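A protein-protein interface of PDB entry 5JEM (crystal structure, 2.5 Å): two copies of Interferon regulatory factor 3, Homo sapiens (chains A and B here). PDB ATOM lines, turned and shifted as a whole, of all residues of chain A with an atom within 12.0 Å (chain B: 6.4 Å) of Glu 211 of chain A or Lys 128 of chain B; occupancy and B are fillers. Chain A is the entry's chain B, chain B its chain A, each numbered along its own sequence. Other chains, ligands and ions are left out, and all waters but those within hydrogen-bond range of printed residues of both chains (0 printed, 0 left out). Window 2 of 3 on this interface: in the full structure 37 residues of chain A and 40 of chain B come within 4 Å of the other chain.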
ATOM      1  N   ASP A 207     -24.365  17.852  -7.769  1.00  0.00           N
ATOM      2  CA  ASP A 207     -23.535  19.036  -7.605  1.00  0.00           C
ATOM      3  C   ASP A 207     -23.498  19.429  -6.135  1.00  0.00           C
ATOM      4  O   ASP A 207     -24.438  20.037  -5.624  1.00  0.00           O
ATOM      5  CB  ASP A 207     -24.066  20.190  -8.457  1.00  0.00           C
ATOM      6  CG  ASP A 207     -23.041  21.289  -8.657  1.00  0.00           C
ATOM      7  OD1 ASP A 207     -22.043  21.323  -7.907  1.00  0.00           O
ATOM      8  OD2 ASP A 207     -23.239  22.123  -9.564  1.00  0.00           O
ATOM      9  N   LEU A 208     -22.413  19.069  -5.458  1.00  0.00           N
ATOM     10  CA  LEU A 208     -22.262  19.390  -4.045  1.00  0.00           C
ATOM     11  C   LEU A 208     -22.027  20.884  -3.844  1.00  0.00           C
ATOM     12  O   LEU A 208     -21.102  21.462  -4.417  1.00  0.00           O
ATOM     13  CB  LEU A 208     -21.112  18.588  -3.432  1.00  0.00           C
ATOM     14  CG  LEU A 208     -21.342  17.081  -3.284  1.00  0.00           C
ATOM     15  CD1 LEU A 208     -20.138  16.411  -2.642  1.00  0.00           C
ATOM     16  CD2 LEU A 208     -22.606  16.805  -2.479  1.00  0.00           C
ATOM     17  N   HIS A 209     -22.880  21.503  -3.034  1.00  0.00           N
ATOM     18  CA  HIS A 209     -22.745  22.917  -2.705  1.00  0.00           C
ATOM     19  C   HIS A 209     -21.927  23.083  -1.432  1.00  0.00           C
ATOM     20  O   HIS A 209     -22.470  23.311  -0.352  1.00  0.00           O
ATOM     21  CB  HIS A 209     -24.119  23.574  -2.546  1.00  0.00           C
ATOM     22  CG  HIS A 209     -24.839  23.793  -3.841  1.00  0.00           C
ATOM     23  ND1 HIS A 209     -25.744  24.815  -4.026  1.00  0.00           N
ATOM     24  CD2 HIS A 209     -24.788  23.119  -5.015  1.00  0.00           C
ATOM     25  CE1 HIS A 209     -26.219  24.764  -5.257  1.00  0.00           C
ATOM     26  NE2 HIS A 209     -25.656  23.744  -5.879  1.00  0.00           N
ATOM     27  N   ILE A 210     -20.614  22.953  -1.571  1.00  0.00           N
ATOM     28  CA  ILE A 210     -19.706  23.035  -0.438  1.00  0.00           C
ATOM     29  C   ILE A 210     -18.594  24.031  -0.732  1.00  0.00           C
ATOM     30  O   ILE A 210     -18.014  24.010  -1.816  1.00  0.00           O
ATOM     31  CB  ILE A 210     -19.098  21.655  -0.107  1.00  0.00           C
ATOM     32  CG1 ILE A 210     -20.206  20.612   0.056  1.00  0.00           C
ATOM     33  CG2 ILE A 210     -18.243  21.735   1.145  1.00  0.00           C
ATOM     34  CD1 ILE A 210     -19.700  19.200   0.257  1.00  0.00           C
ATOM     35  N   GLU A 211     -18.316  24.911   0.227  1.00  0.00           N
ATOM     36  CA  GLU A 211     -17.261  25.911   0.079  1.00  0.00           C
ATOM     37  C   GLU A 211     -15.937  25.263  -0.284  1.00  0.00           C
ATOM     38  O   GLU A 211     -15.497  24.314   0.366  1.00  0.00           O
ATOM     39  CB  GLU A 211     -17.098  26.729   1.361  1.00  0.00           C
ATOM     40  CG  GLU A 211     -18.126  27.829   1.535  1.00  0.00           C
ATOM     41  CD  GLU A 211     -17.859  28.680   2.764  1.00  0.00           C
ATOM     42  OE1 GLU A 211     -17.018  28.278   3.596  1.00  0.00           O
ATOM     43  OE2 GLU A 211     -18.489  29.751   2.896  1.00  0.00           O
ATOM     44  N   ASN A 212     -15.310  25.777  -1.332  1.00  0.00           N
ATOM     45  CA  ASN A 212     -14.061  25.221  -1.812  1.00  0.00           C
ATOM     46  C   ASN A 212     -13.008  26.311  -1.965  1.00  0.00           C
ATOM     47  O   ASN A 212     -11.941  26.084  -2.531  1.00  0.00           O
ATOM     48  CB  ASN A 212     -14.281  24.497  -3.137  1.00  0.00           C
ATOM     49  CG  ASN A 212     -13.226  23.447  -3.411  1.00  0.00           C
ATOM     50  OD1 ASN A 212     -12.885  22.649  -2.537  1.00  0.00           O
ATOM     51  ND2 ASN A 212     -12.694  23.448  -4.626  1.00  0.00           N
ATOM     52  N   SER A 213     -13.322  27.498  -1.455  1.00  0.00           N
ATOM     53  CA  SER A 213     -12.404  28.630  -1.503  1.00  0.00           C
ATOM     54  C   SER A 213     -12.263  29.280  -0.133  1.00  0.00           C
ATOM     55  O   SER A 213     -13.027  28.998   0.787  1.00  0.00           O
ATOM     56  CB  SER A 213     -12.878  29.665  -2.522  1.00  0.00           C
ATOM     57  OG  SER A 213     -12.954  29.099  -3.816  1.00  0.00           O
ATOM     58  OXT SER A 213     -11.382  30.110   0.082  1.00  0.00           O
ATOM     59  N   CYS B  82     -17.998  18.057   6.115  1.00  0.00           N
ATOM     60  CA  CYS B  82     -17.815  19.478   5.861  1.00  0.00           C
ATOM     61  C   CYS B  82     -18.766  20.345   6.679  1.00  0.00           C
ATOM     62  O   CYS B  82     -18.758  21.571   6.557  1.00  0.00           O
ATOM     63  CB  CYS B  82     -17.990  19.765   4.374  1.00  0.00           C
ATOM     64  SG  CYS B  82     -16.788  18.914   3.341  1.00  0.00           S
ATOM     65  N   GLN B  99     -28.000  29.664  11.382  1.00  0.00           N
ATOM     66  CA  GLN B  99     -26.723  30.155  10.886  1.00  0.00           C
ATOM     67  C   GLN B  99     -25.859  28.980  10.449  1.00  0.00           C
ATOM     68  O   GLN B  99     -25.759  27.975  11.154  1.00  0.00           O
ATOM     69  CB  GLN B  99     -26.009  30.985  11.953  1.00  0.00           C
ATOM     70  CG  GLN B  99     -24.745  31.667  11.461  1.00  0.00           C
ATOM     71  CD  GLN B  99     -24.192  32.668  12.458  1.00  0.00           C
ATOM     72  OE1 GLN B  99     -23.186  33.323  12.197  1.00  0.00           O
ATOM     73  NE2 GLN B  99     -24.850  32.793  13.605  1.00  0.00           N
ATOM     74  N   ARG B 100     -25.250  29.103   9.275  1.00  0.00           N
ATOM     75  CA  ARG B 100     -24.393  28.046   8.753  1.00  0.00           C
ATOM     76  C   ARG B 100     -22.947  28.303   9.155  1.00  0.00           C
ATOM     77  O   ARG B 100     -22.331  29.259   8.691  1.00  0.00           O
ATOM     78  CB  ARG B 100     -24.524  27.951   7.232  1.00  0.00           C
ATOM     79  CG  ARG B 100     -23.801  26.768   6.631  1.00  0.00           C
ATOM     80  CD  ARG B 100     -22.590  27.211   5.834  1.00  0.00           C
ATOM     81  NE  ARG B 100     -22.966  28.078   4.723  1.00  0.00           N
ATOM     82  CZ  ARG B 100     -22.108  28.554   3.829  1.00  0.00           C
ATOM     83  NH1 ARG B 100     -20.823  28.242   3.916  1.00  0.00           N
ATOM     84  NH2 ARG B 100     -22.534  29.337   2.847  1.00  0.00           N
ATOM     85  N   LEU B 101     -22.410  27.446  10.019  1.00  0.00           N
ATOM     86  CA  LEU B 101     -21.089  27.673  10.602  1.00  0.00           C
ATOM     87  C   LEU B 101     -19.968  26.935   9.874  1.00  0.00           C
ATOM     88  O   LEU B 101     -18.793  27.248  10.062  1.00  0.00           O
ATOM     89  CB  LEU B 101     -21.084  27.266  12.077  1.00  0.00           C
ATOM     90  CG  LEU B 101     -22.143  27.899  12.979  1.00  0.00           C
ATOM     91  CD1 LEU B 101     -21.965  27.428  14.414  1.00  0.00           C
ATOM     92  CD2 LEU B 101     -22.102  29.416  12.897  1.00  0.00           C
ATOM     93  N   GLY B 102     -20.329  25.958   9.048  1.00  0.00           N
ATOM     94  CA  GLY B 102     -19.344  25.153   8.346  1.00  0.00           C
ATOM     95  C   GLY B 102     -19.227  25.470   6.868  1.00  0.00           C
ATOM     96  O   GLY B 102     -19.468  26.600   6.448  1.00  0.00           O
ATOM     97  N   HIS B 103     -18.864  24.466   6.075  1.00  0.00           N
ATOM     98  CA  HIS B 103     -18.625  24.664   4.646  1.00  0.00           C
ATOM     99  C   HIS B 103     -19.810  24.236   3.773  1.00  0.00           C
ATOM    100  O   HIS B 103     -19.818  24.484   2.565  1.00  0.00           O
ATOM    101  CB  HIS B 103     -17.369  23.902   4.213  1.00  0.00           C
ATOM    102  CG  HIS B 103     -16.138  24.282   4.972  1.00  0.00           C
ATOM    103  ND1 HIS B 103     -15.454  25.461   4.744  1.00  0.00           N
ATOM    104  CD2 HIS B 103     -15.459  23.646   5.957  1.00  0.00           C
ATOM    105  CE1 HIS B 103     -14.416  25.530   5.553  1.00  0.00           C
ATOM    106  NE2 HIS B 103     -14.394  24.440   6.300  1.00  0.00           N
ATOM    107  N   CYS B 104     -20.806  23.597   4.379  1.00  0.00           N
ATOM    108  CA  CYS B 104     -21.954  23.097   3.627  1.00  0.00           C
ATOM    109  C   CYS B 104     -23.044  24.148   3.455  1.00  0.00           C
ATOM    110  O   CYS B 104     -23.688  24.541   4.425  1.00  0.00           O
ATOM    111  CB  CYS B 104     -22.551  21.863   4.310  1.00  0.00           C
ATOM    112  SG  CYS B 104     -21.528  20.380   4.234  1.00  0.00           S
ATOM    113  N   HIS B 105     -23.250  24.595   2.218  1.00  0.00           N
ATOM    114  CA  HIS B 105     -24.375  25.468   1.906  1.00  0.00           C
ATOM    115  C   HIS B 105     -25.670  24.783   2.320  1.00  0.00           C
ATOM    116  O   HIS B 105     -25.847  23.583   2.106  1.00  0.00           O
ATOM    117  CB  HIS B 105     -24.408  25.816   0.418  1.00  0.00           C
ATOM    118  CG  HIS B 105     -23.333  26.767  -0.003  1.00  0.00           C
ATOM    119  ND1 HIS B 105     -23.563  28.115  -0.187  1.00  0.00           N
ATOM    120  CD2 HIS B 105     -22.023  26.570  -0.276  1.00  0.00           C
ATOM    121  CE1 HIS B 105     -22.442  28.705  -0.555  1.00  0.00           C
ATOM    122  NE2 HIS B 105     -21.489  27.790  -0.617  1.00  0.00           N
ATOM    123  N   VAL B 126     -29.632  29.628   4.385  1.00  0.00           N
ATOM    124  CA  VAL B 126     -29.151  29.967   5.715  1.00  0.00           C
ATOM    125  C   VAL B 126     -27.822  30.716   5.616  1.00  0.00           C
ATOM    126  O   VAL B 126     -26.867  30.219   5.023  1.00  0.00           O
ATOM    127  CB  VAL B 126     -28.978  28.709   6.581  1.00  0.00           C
ATOM    128  CG1 VAL B 126     -28.485  29.083   7.965  1.00  0.00           C
ATOM    129  CG2 VAL B 126     -30.291  27.942   6.665  1.00  0.00           C
ATOM    130  N   PRO B 127     -27.767  31.929   6.184  1.00  0.00           N
ATOM    131  CA  PRO B 127     -26.562  32.765   6.122  1.00  0.00           C
ATOM    132  C   PRO B 127     -25.414  32.193   6.945  1.00  0.00           C
ATOM    133  O   PRO B 127     -25.643  31.347   7.813  1.00  0.00           O
ATOM    134  CB  PRO B 127     -27.032  34.103   6.696  1.00  0.00           C
ATOM    135  CG  PRO B 127     -28.192  33.756   7.559  1.00  0.00           C
ATOM    136  CD  PRO B 127     -28.870  32.599   6.894  1.00  0.00           C
ATOM    137  N   LYS B 128     -24.195  32.647   6.668  1.00  0.00           N
ATOM    138  CA  LYS B 128     -23.014  32.159   7.372  1.00  0.00           C
ATOM    139  C   LYS B 128     -22.395  33.220   8.273  1.00  0.00           C
ATOM    140  O   LYS B 128     -22.142  32.971   9.449  1.00  0.00           O
ATOM    141  CB  LYS B 128     -21.962  31.660   6.381  1.00  0.00           C
ATOM    142  CG  LYS B 128     -20.612  31.393   7.024  1.00  0.00           C
ATOM    143  CD  LYS B 128     -19.624  30.771   6.058  1.00  0.00           C
ATOM    144  CE  LYS B 128     -18.327  30.424   6.770  1.00  0.00           C
ATOM    145  NZ  LYS B 128     -17.313  29.835   5.853  1.00  0.00           N
ATOM    146  N   ASP B 129     -22.149  34.401   7.712  1.00  0.00           N
ATOM    147  CA  ASP B 129     -21.456  35.471   8.429  1.00  0.00           C
ATOM    148  C   ASP B 129     -22.287  36.039   9.573  1.00  0.00           C
ATOM    149  O   ASP B 129     -21.749  36.617  10.518  1.00  0.00           O
ATOM    150  CB  ASP B 129     -21.073  36.592   7.461  1.00  0.00           C
ATOM    151  CG  ASP B 129     -20.214  36.102   6.312  1.00  0.00           C
ATOM    152  OD1 ASP B 129     -19.444  35.136   6.509  1.00  0.00           O
ATOM    153  OD2 ASP B 129     -20.310  36.682   5.211  1.00  0.00           O
ATOM    154  N   LYS B 130     -23.599  35.872   9.479  1.00  0.00           N
ATOM    155  CA  LYS B 130     -24.519  36.368  10.492  1.00  0.00           C
ATOM    156  C   LYS B 130     -25.733  35.448  10.558  1.00  0.00           C
ATOM    157  O   LYS B 130     -25.920  34.607   9.681  1.00  0.00           O
ATOM    158  CB  LYS B 130     -24.938  37.805  10.176  1.00  0.00           C
ATOM    159  CG  LYS B 130     -25.634  37.962   8.831  1.00  0.00           C
ATOM    160  CD  LYS B 130     -25.495  39.375   8.280  1.00  0.00           C
ATOM    161  CE  LYS B 130     -24.059  39.672   7.867  1.00  0.00           C
ATOM    162  NZ  LYS B 130     -23.950  40.929   7.073  1.00  0.00           N
ATOM    163  N   GLU B 131     -26.552  35.596  11.594  1.00  0.00           N
ATOM    164  CA  GLU B 131     -27.743  34.764  11.717  1.00  0.00           C
ATOM    165  C   GLU B 131     -28.877  35.316  10.865  1.00  0.00           C
ATOM    166  O   GLU B 131     -28.885  36.492  10.509  1.00  0.00           O
ATOM    167  CB  GLU B 131     -28.193  34.654  13.177  1.00  0.00           C
ATOM    168  CG  GLU B 131     -28.753  35.941  13.767  1.00  0.00           C
ATOM    169  CD  GLU B 131     -27.677  36.848  14.332  1.00  0.00           C
ATOM    170  OE1 GLU B 131     -28.000  38.008  14.666  1.00  0.00           O
ATOM    171  OE2 GLU B 131     -26.516  36.400  14.452  1.00  0.00           O
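His 209 of chain A touches Cys 104 of chain B (O to C, 3.9 Å). Cys 82 of chain B touches Ile 210 of chain A. CA of Ile 210 of chain A touches O of His 103 of chain B (3.3 Å). Glu 211 of chain A touches His 105 of chain B.
The guanidinium group (NH1) of Arg 100 of chain B lies within salt-bridge range of the side-chain carboxylate (OE2) of Glu 211 of chain A (3.0 Å). N of Glu 211 of chain A is in hydrogen-bond range of O of His 103 of chain B (2.8 Å). The backbone carbonyl oxygen (O) of His 209 of chain A is in hydrogen-bond range of the backbone NH (N) of His 105 of chain B, 3.0 Å away. The side-chain amino group (NZ) of Lys 128 of chain B lies within salt-bridge range of the side-chain carboxylate (OE1) of Glu 211 of chain A, at 2.8 Å.
Printed residues of chain A within 4 Å of Lys 128 of chain B: Glu 211 (2.8 Å). No residue of chain A comes within 4 Å of Gln 99 of chain B. Arg 100 of chain B touches just one residue of chain A: Glu 211. No residue of chain A comes within 4 Å of Gly 102 of chain B. No residue of chain A comes within 4 Å of Pro 127 of chain B. No residue of chain A comes within 4 Å of Asp 129 of chain B. Of the printed residues of chain A, Cys 82 of chain B touches Ile 210. Of the printed residues of chain B, His 209 of chain A touches Cys 104 and His 105. Leu 208 of chain A touches none of the printed residues of chain B.
The backbone NH (N) of His 103 of chain B is in hydrogen-bond range of the backbone carbonyl oxygen (O) of Cys 82 of chain B (2.9 Å). The backbone carbonyl oxygen of Lys 128 of chain B lies close to the side-chain amide oxygen of Gln 99 of chain B (3.0 Å). The guanidinium group (NH1) of Arg 100 of chain B lies close to the backbone carbonyl oxygen (O) of Gly 102 of chain B (3.3 Å). The guanidinium group (NH2) of Arg 100 of chain B sits at hydrogen-bond distance from a ring nitrogen (ND1) of His 105 of chain B, at 3.4 Å. The backbone NH of Arg 100 of chain B is in hydrogen-bond range of the backbone carbonyl oxygen of Pro 127 of chain B (2.7 Å).
No position is printed for both chains.
Printed residues of chain A that touch a printed residue of chain B: His 209, Ile 210 and Glu 211. Of the 14 printed residues of chain B, 6 touch a printed residue of chain A. Along chain B the printed residues that touch a printed residue of chain A span positions 82 to 128. Among the printed residues, Asp or Glu carboxylates within 4 Å of a Lys or Arg side-chain nitrogen of the other chain: Glu 211 of chain A with Arg 100 of chain B and Glu 211 of chain A with Lys 128 of chain B.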
